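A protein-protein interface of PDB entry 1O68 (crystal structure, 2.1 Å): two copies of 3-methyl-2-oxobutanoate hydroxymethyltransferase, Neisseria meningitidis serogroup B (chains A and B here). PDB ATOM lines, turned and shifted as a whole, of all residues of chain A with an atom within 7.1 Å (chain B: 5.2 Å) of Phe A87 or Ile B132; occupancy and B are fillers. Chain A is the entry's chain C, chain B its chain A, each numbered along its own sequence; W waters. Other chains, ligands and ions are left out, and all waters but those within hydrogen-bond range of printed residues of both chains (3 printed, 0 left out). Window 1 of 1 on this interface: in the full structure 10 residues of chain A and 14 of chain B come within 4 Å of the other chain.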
ATOM      1  N   ASP A  45       6.969  13.205   5.370  1.00  0.00           N
ATOM      2  CA  ASP A  45       5.616  13.658   5.086  1.00  0.00           C
ATOM      3  C   ASP A  45       5.191  14.726   6.101  1.00  0.00           C
ATOM      4  O   ASP A  45       4.155  15.369   5.959  1.00  0.00           O
ATOM      5  CB  ASP A  45       4.624  12.522   4.993  1.00  0.00           C
ATOM      6  CG  ASP A  45       4.418  11.801   6.319  1.00  0.00           C
ATOM      7  OD1 ASP A  45       5.160  12.076   7.272  1.00  0.00           O
ATOM      8  OD2 ASP A  45       3.478  10.995   6.402  1.00  0.00           O
ATOM      9  N   THR A  57      -0.442  14.834   8.182  1.00  0.00           N
ATOM     10  CA  THR A  57       0.357  14.503   7.017  1.00  0.00           C
ATOM     11  C   THR A  57      -0.436  13.642   6.040  1.00  0.00           C
ATOM     12  O   THR A  57       0.131  13.274   5.008  1.00  0.00           O
ATOM     13  CB  THR A  57       1.630  13.707   7.419  1.00  0.00           C
ATOM     14  OG1 THR A  57       1.201  12.442   7.940  1.00  0.00           O
ATOM     15  CG2 THR A  57       2.410  14.413   8.519  1.00  0.00           C
ATOM     16  N   LEU A  58      -1.703  13.320   6.325  1.00  0.00           N
ATOM     17  CA  LEU A  58      -2.457  12.438   5.430  1.00  0.00           C
ATOM     18  C   LEU A  58      -2.698  12.987   4.044  1.00  0.00           C
ATOM     19  O   LEU A  58      -2.583  12.227   3.093  1.00  0.00           O
ATOM     20  CB  LEU A  58      -3.732  11.891   6.053  1.00  0.00           C
ATOM     21  CG  LEU A  58      -3.550  10.793   7.104  1.00  0.00           C
ATOM     22  CD1 LEU A  58      -2.982  11.345   8.414  1.00  0.00           C
ATOM     23  CD2 LEU A  58      -4.865  10.084   7.380  1.00  0.00           C
ATOM     24  N   PRO A  59      -2.982  14.271   3.854  1.00  0.00           N
ATOM     25  CA  PRO A  59      -3.203  14.840   2.532  1.00  0.00           C
ATOM     26  C   PRO A  59      -1.974  14.930   1.650  1.00  0.00           C
ATOM     27  O   PRO A  59      -2.063  15.301   0.446  1.00  0.00           O
ATOM     28  CB  PRO A  59      -3.853  16.187   2.796  1.00  0.00           C
ATOM     29  CG  PRO A  59      -4.278  16.163   4.241  1.00  0.00           C
ATOM     30  CD  PRO A  59      -3.313  15.233   4.933  1.00  0.00           C
ATOM     31  N   VAL A  60      -0.769  14.715   2.162  1.00  0.00           N
ATOM     32  CA  VAL A  60       0.452  14.746   1.367  1.00  0.00           C
ATOM     33  C   VAL A  60       0.375  13.680   0.278  1.00  0.00           C
ATOM     34  O   VAL A  60       0.184  12.501   0.589  1.00  0.00           O
ATOM     35  CB  VAL A  60       1.687  14.533   2.249  1.00  0.00           C
ATOM     36  CG1 VAL A  60       2.984  14.490   1.419  1.00  0.00           C
ATOM     37  CG2 VAL A  60       1.812  15.677   3.260  1.00  0.00           C
ATOM     38  N   SER A  61       0.622  14.041  -0.978  1.00  0.00           N
ATOM     39  CA  SER A  61       0.556  13.140  -2.091  1.00  0.00           C
ATOM     40  C   SER A  61       1.927  12.645  -2.543  1.00  0.00           C
ATOM     41  O   SER A  61       2.977  13.212  -2.231  1.00  0.00           O
ATOM     42  CB  SER A  61      -0.105  13.819  -3.312  1.00  0.00           C
ATOM     43  OG  SER A  61       0.749  14.834  -3.822  1.00  0.00           O
ATOM     44  N   LEU A  62       1.894  11.610  -3.383  1.00  0.00           N
ATOM     45  CA  LEU A  62       3.113  11.037  -3.929  1.00  0.00           C
ATOM     46  C   LEU A  62       3.830  12.097  -4.769  1.00  0.00           C
ATOM     47  O   LEU A  62       5.048  12.189  -4.758  1.00  0.00           O
ATOM     48  CB  LEU A  62       2.804   9.810  -4.807  1.00  0.00           C
ATOM     49  CG  LEU A  62       4.018   9.152  -5.451  1.00  0.00           C
ATOM     50  CD1 LEU A  62       5.049   8.785  -4.390  1.00  0.00           C
ATOM     51  CD2 LEU A  62       3.629   7.910  -6.259  1.00  0.00           C
ATOM     52  N   MET A  65       5.784  14.363  -2.499  1.00  0.00           N
ATOM     53  CA  MET A  65       7.014  13.722  -2.011  1.00  0.00           C
ATOM     54  C   MET A  65       8.074  13.673  -3.098  1.00  0.00           C
ATOM     55  O   MET A  65       9.246  13.978  -2.856  1.00  0.00           O
ATOM     56  CB  MET A  65       6.696  12.342  -1.451  1.00  0.00           C
ATOM     57  CG  MET A  65       5.721  12.318  -0.266  1.00  0.00           C
ATOM     58  SD  MET A  65       6.323  13.436   1.208  1.00  0.00           S
ATOM     59  CE  MET A  65       8.179  12.973   1.171  1.00  0.00           C
ATOM     60  N   ASP A  84       9.948   9.772   2.570  1.00  0.00           N
ATOM     61  CA  ASP A  84       8.772   9.091   3.068  1.00  0.00           C
ATOM     62  C   ASP A  84       7.818   8.661   1.941  1.00  0.00           C
ATOM     63  O   ASP A  84       7.641   9.376   0.965  1.00  0.00           O
ATOM     64  CB  ASP A  84       7.940  10.049   3.934  1.00  0.00           C
ATOM     65  CG  ASP A  84       8.212   9.927   5.405  1.00  0.00           C
ATOM     66  OD1 ASP A  84       8.700   8.862   5.825  1.00  0.00           O
ATOM     67  OD2 ASP A  84       7.925  10.915   6.117  1.00  0.00           O
ATOM     68  N   LEU A  85       7.212   7.494   2.142  1.00  0.00           N
ATOM     69  CA  LEU A  85       6.162   7.017   1.238  1.00  0.00           C
ATOM     70  C   LEU A  85       4.902   7.665   1.901  1.00  0.00           C
ATOM     71  O   LEU A  85       4.813   7.540   3.123  1.00  0.00           O
ATOM     72  CB  LEU A  85       6.011   5.505   1.288  1.00  0.00           C
ATOM     73  CG  LEU A  85       7.144   4.701   0.628  1.00  0.00           C
ATOM     74  CD1 LEU A  85       6.935   3.218   0.845  1.00  0.00           C
ATOM     75  CD2 LEU A  85       7.210   5.022  -0.866  1.00  0.00           C
ATOM     76  N   PRO A  86       4.188   8.502   1.185  1.00  0.00           N
ATOM     77  CA  PRO A  86       3.050   9.243   1.738  1.00  0.00           C
ATOM     78  C   PRO A  86       1.810   8.417   1.944  1.00  0.00           C
ATOM     79  O   PRO A  86       1.613   7.369   1.302  1.00  0.00           O
ATOM     80  CB  PRO A  86       2.860  10.351   0.700  1.00  0.00           C
ATOM     81  CG  PRO A  86       3.242   9.718  -0.585  1.00  0.00           C
ATOM     82  CD  PRO A  86       4.307   8.690  -0.277  1.00  0.00           C
ATOM     83  N   PHE A  87       0.971   8.807   2.903  1.00  0.00           N
ATOM     84  CA  PHE A  87      -0.244   8.081   3.246  1.00  0.00           C
ATOM     85  C   PHE A  87      -1.112   7.822   2.031  1.00  0.00           C
ATOM     86  O   PHE A  87      -1.352   8.761   1.286  1.00  0.00           O
ATOM     87  CB  PHE A  87      -1.100   8.862   4.274  1.00  0.00           C
ATOM     88  CG  PHE A  87      -2.466   8.232   4.474  1.00  0.00           C
ATOM     89  CD1 PHE A  87      -2.614   7.198   5.377  1.00  0.00           C
ATOM     90  CD2 PHE A  87      -3.572   8.664   3.770  1.00  0.00           C
ATOM     91  CE1 PHE A  87      -3.849   6.587   5.580  1.00  0.00           C
ATOM     92  CE2 PHE A  87      -4.809   8.070   3.970  1.00  0.00           C
ATOM     93  CZ  PHE A  87      -4.939   7.019   4.864  1.00  0.00           C
ATOM     94  N   GLY A  88      -1.571   6.585   1.849  1.00  0.00           N
ATOM     95  CA  GLY A  88      -2.414   6.229   0.728  1.00  0.00           C
ATOM     96  C   GLY A  88      -1.661   5.783  -0.514  1.00  0.00           C
ATOM     97  O   GLY A  88      -2.209   5.042  -1.339  1.00  0.00           O
ATOM     98  N   ALA A  89      -0.357   6.081  -0.574  1.00  0.00           N
ATOM     99  CA  ALA A  89       0.455   5.734  -1.725  1.00  0.00           C
ATOM    100  C   ALA A  89       1.160   4.387  -1.664  1.00  0.00           C
ATOM    101  O   ALA A  89       1.677   3.946  -2.705  1.00  0.00           O
ATOM    102  CB  ALA A  89       1.533   6.823  -1.898  1.00  0.00           C
ATOM    103  N   TYR A  90       1.161   3.670  -0.554  1.00  0.00           N
ATOM    104  CA  TYR A  90       1.873   2.414  -0.471  1.00  0.00           C
ATOM    105  C   TYR A  90       1.244   1.317   0.355  1.00  0.00           C
ATOM    106  O   TYR A  90       1.727   0.167   0.282  1.00  0.00           O
ATOM    107  CB  TYR A  90       3.287   2.675   0.137  1.00  0.00           C
ATOM    108  CG  TYR A  90       3.226   3.138   1.572  1.00  0.00           C
ATOM    109  CD1 TYR A  90       2.846   4.443   1.898  1.00  0.00           C
ATOM    110  CD2 TYR A  90       3.532   2.271   2.612  1.00  0.00           C
ATOM    111  CE1 TYR A  90       2.789   4.857   3.220  1.00  0.00           C
ATOM    112  CE2 TYR A  90       3.482   2.676   3.920  1.00  0.00           C
ATOM    113  CZ  TYR A  90       3.098   3.971   4.220  1.00  0.00           C
ATOM    114  OH  TYR A  90       3.054   4.358   5.538  1.00  0.00           O
ATOM    115  N   GLN A  91       0.165   1.580   1.082  1.00  0.00           N
ATOM    116  CA  GLN A  91      -0.435   0.569   1.930  1.00  0.00           C
ATOM    117  C   GLN A  91      -1.420  -0.342   1.227  1.00  0.00           C
ATOM    118  O   GLN A  91      -1.865  -1.323   1.838  1.00  0.00           O
ATOM    119  CB  GLN A  91      -1.115   1.217   3.148  1.00  0.00           C
ATOM    120  CG  GLN A  91      -0.216   2.146   3.937  1.00  0.00           C
ATOM    121  CD  GLN A  91      -0.396   3.610   3.603  1.00  0.00           C
ATOM    122  OE1 GLN A  91      -0.602   4.039   2.453  1.00  0.00           O
ATOM    123  NE2 GLN A  91      -0.284   4.419   4.657  1.00  0.00           N
ATOM    124  N   GLU A 115       5.642   3.458   7.224  1.00  0.00           N
ATOM    125  CA  GLU A 115       5.120   3.344   8.575  1.00  0.00           C
ATOM    126  C   GLU A 115       4.327   2.059   8.760  1.00  0.00           C
ATOM    127  O   GLU A 115       3.599   1.678   7.852  1.00  0.00           O
ATOM    128  CB  GLU A 115       4.197   4.552   8.877  1.00  0.00           C
ATOM    129  CG  GLU A 115       4.909   5.902   8.898  1.00  0.00           C
ATOM    130  CD  GLU A 115       4.029   7.054   9.350  1.00  0.00           C
ATOM    131  OE1 GLU A 115       4.472   8.222   9.338  1.00  0.00           O
ATOM    132  OE2 GLU A 115       2.873   6.864   9.789  1.00  0.00           O
ATOM    133  N   GLN A 143       0.934   8.877  10.423  1.00  0.00           N
ATOM    134  CA  GLN A 143      -0.048   8.583   9.382  1.00  0.00           C
ATOM    135  C   GLN A 143      -1.266   7.884   9.955  1.00  0.00           C
ATOM    136  O   GLN A 143      -2.317   7.868   9.316  1.00  0.00           O
ATOM    137  CB  GLN A 143       0.547   7.771   8.235  1.00  0.00           C
ATOM    138  CG  GLN A 143       1.477   8.613   7.366  1.00  0.00           C
ATOM    139  CD  GLN A 143       2.197   7.787   6.322  1.00  0.00           C
ATOM    140  OE1 GLN A 143       1.749   6.682   6.002  1.00  0.00           O
ATOM    141  NE2 GLN A 143       3.327   8.310   5.842  1.00  0.00           N
ATOM    142  N   SER A 144      -1.138   7.254  11.124  1.00  0.00           N
ATOM    143  CA  SER A 144      -2.296   6.609  11.734  1.00  0.00           C
ATOM    144  C   SER A 144      -2.788   7.441  12.921  1.00  0.00           C
ATOM    145  O   SER A 144      -3.503   6.934  13.778  1.00  0.00           O
ATOM    146  CB  SER A 144      -1.977   5.176  12.177  1.00  0.00           C
ATOM    147  OG  SER A 144      -1.136   5.238  13.334  1.00  0.00           O
ATOM    148  N   PHE A 146      -5.314   9.463  13.202  1.00  0.00           N
ATOM    149  CA  PHE A 146      -6.755   9.462  13.435  1.00  0.00           C
ATOM    150  C   PHE A 146      -7.230   8.159  14.041  1.00  0.00           C
ATOM    151  O   PHE A 146      -8.324   8.106  14.582  1.00  0.00           O
ATOM    152  CB  PHE A 146      -7.521   9.813  12.153  1.00  0.00           C
ATOM    153  CG  PHE A 146      -7.264  11.230  11.683  1.00  0.00           C
ATOM    154  CD1 PHE A 146      -6.550  11.479  10.533  1.00  0.00           C
ATOM    155  CD2 PHE A 146      -7.727  12.307  12.424  1.00  0.00           C
ATOM    156  CE1 PHE A 146      -6.311  12.763  10.090  1.00  0.00           C
ATOM    157  CE2 PHE A 146      -7.487  13.599  12.011  1.00  0.00           C
ATOM    158  CZ  PHE A 146      -6.787  13.832  10.827  1.00  0.00           C
ATOM    159  N   ALA A 147      -6.466   7.082  13.937  1.00  0.00           N
ATOM    160  CA  ALA A 147      -6.838   5.790  14.495  1.00  0.00           C
ATOM    161  C   ALA A 147      -6.232   5.636  15.902  1.00  0.00           C
ATOM    162  O   ALA A 147      -6.975   5.836  16.879  1.00  0.00           O
ATOM    163  CB  ALA A 147      -6.388   4.647  13.616  1.00  0.00           C
ATOM    164  N   PHE B  98      -9.791   0.975   0.237  1.00  0.00           N
ATOM    165  CA  PHE B  98      -8.682   1.698   0.872  1.00  0.00           C
ATOM    166  C   PHE B  98      -8.317   2.923   0.025  1.00  0.00           C
ATOM    167  O   PHE B  98      -8.092   4.015   0.575  1.00  0.00           O
ATOM    168  CB  PHE B  98      -7.463   0.777   1.100  1.00  0.00           C
ATOM    169  CG  PHE B  98      -6.274   1.578   1.605  1.00  0.00           C
ATOM    170  CD1 PHE B  98      -6.141   1.841   2.942  1.00  0.00           C
ATOM    171  CD2 PHE B  98      -5.360   2.136   0.718  1.00  0.00           C
ATOM    172  CE1 PHE B  98      -5.171   2.709   3.412  1.00  0.00           C
ATOM    173  CE2 PHE B  98      -4.343   2.938   1.191  1.00  0.00           C
ATOM    174  CZ  PHE B  98      -4.282   3.285   2.533  1.00  0.00           C
ATOM    175  N   ALA B 101     -11.151   5.501   0.482  1.00  0.00           N
ATOM    176  CA  ALA B 101     -11.071   6.056   1.844  1.00  0.00           C
ATOM    177  C   ALA B 101      -9.868   6.957   2.008  1.00  0.00           C
ATOM    178  O   ALA B 101      -9.895   8.026   2.641  1.00  0.00           O
ATOM    179  CB  ALA B 101     -11.051   4.894   2.846  1.00  0.00           C
ATOM    180  N   ALA B 102      -8.730   6.596   1.378  1.00  0.00           N
ATOM    181  CA  ALA B 102      -7.548   7.448   1.446  1.00  0.00           C
ATOM    182  C   ALA B 102      -7.829   8.817   0.822  1.00  0.00           C
ATOM    183  O   ALA B 102      -7.323   9.817   1.337  1.00  0.00           O
ATOM    184  CB  ALA B 102      -6.349   6.815   0.769  1.00  0.00           C
ATOM    185  N   MET B 105      -9.832  10.775   3.354  1.00  0.00           N
ATOM    186  CA  MET B 105      -8.993  11.235   4.474  1.00  0.00           C
ATOM    187  C   MET B 105      -8.149  12.413   3.983  1.00  0.00           C
ATOM    188  O   MET B 105      -7.931  13.410   4.677  1.00  0.00           O
ATOM    189  CB  MET B 105      -8.093  10.138   5.012  1.00  0.00           C
ATOM    190  CG  MET B 105      -8.773   8.902   5.528  1.00  0.00           C
ATOM    191  SD  MET B 105      -9.902   9.171   7.028  1.00  0.00           S
ATOM    192  CE  MET B 105      -8.639   9.710   8.345  1.00  0.00           C
ATOM    193  N   VAL B 112     -14.105   7.159   7.944  1.00  0.00           N
ATOM    194  CA  VAL B 112     -14.963   6.922   6.790  1.00  0.00           C
ATOM    195  C   VAL B 112     -16.118   6.000   7.209  1.00  0.00           C
ATOM    196  O   VAL B 112     -15.965   5.244   8.152  1.00  0.00           O
ATOM    197  CB  VAL B 112     -14.228   6.282   5.611  1.00  0.00           C
ATOM    198  CG1 VAL B 112     -13.167   7.257   5.074  1.00  0.00           C
ATOM    199  CG2 VAL B 112     -13.603   4.952   6.033  1.00  0.00           C
ATOM    200  N   LEU B 127      -8.789  -1.451   6.323  1.00  0.00           N
ATOM    201  CA  LEU B 127      -8.707  -0.003   6.482  1.00  0.00           C
ATOM    202  C   LEU B 127      -8.235   0.426   7.852  1.00  0.00           C
ATOM    203  O   LEU B 127      -7.301   1.224   7.983  1.00  0.00           O
ATOM    204  CB  LEU B 127     -10.101   0.607   6.202  1.00  0.00           C
ATOM    205  CG  LEU B 127     -10.334   1.093   4.763  1.00  0.00           C
ATOM    206  CD1 LEU B 127     -10.054   0.013   3.744  1.00  0.00           C
ATOM    207  CD2 LEU B 127     -11.769   1.601   4.616  1.00  0.00           C
ATOM    208  N   GLN B 128      -8.822  -0.175   8.899  1.00  0.00           N
ATOM    209  CA  GLN B 128      -8.454   0.187  10.273  1.00  0.00           C
ATOM    210  C   GLN B 128      -6.992  -0.092  10.543  1.00  0.00           C
ATOM    211  O   GLN B 128      -6.264   0.732  11.092  1.00  0.00           O
ATOM    212  CB  GLN B 128      -9.354  -0.516  11.284  1.00  0.00           C
ATOM    213  CG  GLN B 128      -9.070  -1.966  11.535  1.00  0.00           C
ATOM    214  CD  GLN B 128      -8.145  -2.267  12.690  1.00  0.00           C
ATOM    215  OE1 GLN B 128      -7.372  -1.424  13.143  1.00  0.00           O
ATOM    216  NE2 GLN B 128      -8.212  -3.502  13.199  1.00  0.00           N
ATOM    217  N   ARG B 130      -4.626   0.119   8.566  1.00  0.00           N
ATOM    218  CA  ARG B 130      -3.856   1.122   7.868  1.00  0.00           C
ATOM    219  C   ARG B 130      -4.102   2.553   8.323  1.00  0.00           C
ATOM    220  O   ARG B 130      -3.885   3.498   7.534  1.00  0.00           O
ATOM    221  CB  ARG B 130      -4.113   0.994   6.342  1.00  0.00           C
ATOM    222  CG  ARG B 130      -3.398  -0.289   5.879  1.00  0.00           C
ATOM    223  CD  ARG B 130      -3.975  -0.864   4.600  1.00  0.00           C
ATOM    224  NE  ARG B 130      -3.145  -2.027   4.209  1.00  0.00           N
ATOM    225  CZ  ARG B 130      -3.258  -3.203   4.805  1.00  0.00           C
ATOM    226  NH1 ARG B 130      -4.158  -3.364   5.775  1.00  0.00           N
ATOM    227  NH2 ARG B 130      -2.487  -4.216   4.439  1.00  0.00           N
ATOM    228  N   GLY B 131      -4.608   2.754   9.532  1.00  0.00           N
ATOM    229  CA  GLY B 131      -4.812   4.087  10.062  1.00  0.00           C
ATOM    230  C   GLY B 131      -6.078   4.785   9.673  1.00  0.00           C
ATOM    231  O   GLY B 131      -6.275   5.959  10.023  1.00  0.00           O
ATOM    232  N   ILE B 132      -6.994   4.099   8.990  1.00  0.00           N
ATOM    233  CA  ILE B 132      -8.247   4.701   8.577  1.00  0.00           C
ATOM    234  C   ILE B 132      -9.389   4.239   9.471  1.00  0.00           C
ATOM    235  O   ILE B 132      -9.820   3.098   9.310  1.00  0.00           O
ATOM    236  CB  ILE B 132      -8.566   4.325   7.103  1.00  0.00           C
ATOM    237  CG1 ILE B 132      -7.465   4.882   6.198  1.00  0.00           C
ATOM    238  CG2 ILE B 132      -9.939   4.850   6.733  1.00  0.00           C
ATOM    239  CD1 ILE B 132      -7.734   4.828   4.715  1.00  0.00           C
ATOM    240  N   PRO B 133      -9.840   5.065  10.391  1.00  0.00           N
ATOM    241  CA  PRO B 133     -10.952   4.714  11.285  1.00  0.00           C
ATOM    242  C   PRO B 133     -12.198   4.444  10.458  1.00  0.00           C
ATOM    243  O   PRO B 133     -12.493   5.142   9.477  1.00  0.00           O
ATOM    244  CB  PRO B 133     -11.123   5.945  12.171  1.00  0.00           C
ATOM    245  CG  PRO B 133      -9.831   6.681  12.045  1.00  0.00           C
ATOM    246  CD  PRO B 133      -9.396   6.467  10.606  1.00  0.00           C
ATOM    247  N   VAL B 134     -12.949   3.414  10.799  1.00  0.00           N
ATOM    248  CA  VAL B 134     -14.128   3.030  10.084  1.00  0.00           C
ATOM    249  C   VAL B 134     -15.394   2.980  10.941  1.00  0.00           C
ATOM    250  O   VAL B 134     -15.461   2.445  12.045  1.00  0.00           O
ATOM    251  CB  VAL B 134     -13.930   1.621   9.446  1.00  0.00           C
ATOM    252  CG1 VAL B 134     -15.265   1.096   8.919  1.00  0.00           C
ATOM    253  CG2 VAL B 134     -12.892   1.651   8.323  1.00  0.00           C
HETATM  254  O   HOH W   1      -0.500  -3.931   2.367  1.00  0.00           O
HETATM  255  O   HOH W   2      -4.475   9.857   0.586  1.00  0.00           O
HETATM  256  O   HOH W   3      -5.128   8.412  10.602  1.00  0.00           O
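The backbone carbonyl oxygen (O) of Pro B133 sits at hydrogen-bond distance from the backbone NH (N) of Val B112.
The backbone NH of Ile B132 lies within hydrogen-bond range of the backbone carbonyl oxygen of Leu B127 (3.1 Å).
NE2 of Gln A91 sits at hydrogen-bond distance from OE1 of Gln A143 (3.3 Å).
The backbone NH of Gly A88 is in hydrogen-bond range of the side-chain amide oxygen of Gln A91 (2.8 Å).
The side-chain hydroxyl (OH) of Tyr A90 sits close to the side-chain amide nitrogen (NE2) of Gln A91 (3.5 Å).
No position is printed for both chains.
Hydrophobic or aromatic side chains of chain B within 4 Å of the printed part of chain A: Phe B98, Ala B102, Met B105, Ile B132 and Pro B133.
Of the 21 printed residues of chain A, 7 touch a printed residue of chain B.
Among the printed residues, no Asp or Glu carboxylate lies within 4 Å of a Lys or Arg side-chain nitrogen of the other chain.
CE of Met B105 touches CD2 of Leu A58, 3.9 Å away.
Ala B102 touches Phe A87.
Phe A87 touches Arg B130.
CE2 of Phe B98 touches CA of Gly A88 (3.8 Å).
CA of Gly A88 touches CB of Ala B102, at 3.98 Å.
Gln A91 touches Phe B98.
Ser A144 touches Gly B131 (CB to CA, 3.7 Å).
Met B105 touches Phe A146.
Pro B133 touches Phe A146 (CG to O, 3.3 Å).
Ala A147 touches Pro B133 (N to CG, 3.9 Å).
The backbone carbonyl oxygen (O) of Gln A91 sits at hydrogen-bond distance from the guanidinium group (NE) of Arg B130 (2.8 Å).
Water W3 lies within hydrogen-bond range of the backbone carbonyl oxygen (O) of Gly B131 (2.8 Å), the backbone NH (N) of Phe A146 (2.8 Å) and the backbone carbonyl oxygen (O) of Gln A143 (3.1 Å).
Water W1 bridges NH2 of Arg B130 and O of Gln A91.
Water W2 bridges O of Ala B102 (2.9 Å) and O of Phe A87 (3.4 Å).
Of the printed residues of chain B, Phe A87 touches Ala B102 (3.8 Å), Arg B130 (3.7 Å) and Ile B132 (3.6 Å).
Printed residues of chain B within 4 Å of Ser A144: Gly B131.
Of the printed residues of chain A, Arg B130 touches Phe A87 (3.7 Å) and Gln A91 (2.8 Å).
Printed residues of chain B within 4 Å of Gly A88: Phe B98 and Ala B102.
The nearest printed residue of chain B that does not touch Phe A87 is Met B105 (4.02 Å).
The nearest residue of chain A that does not touch Ile B132 is Ala A147 (4.7 Å).
The nearest printed residue of chain B that does not touch Ala A147 is Gln B128 (4.7 Å).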
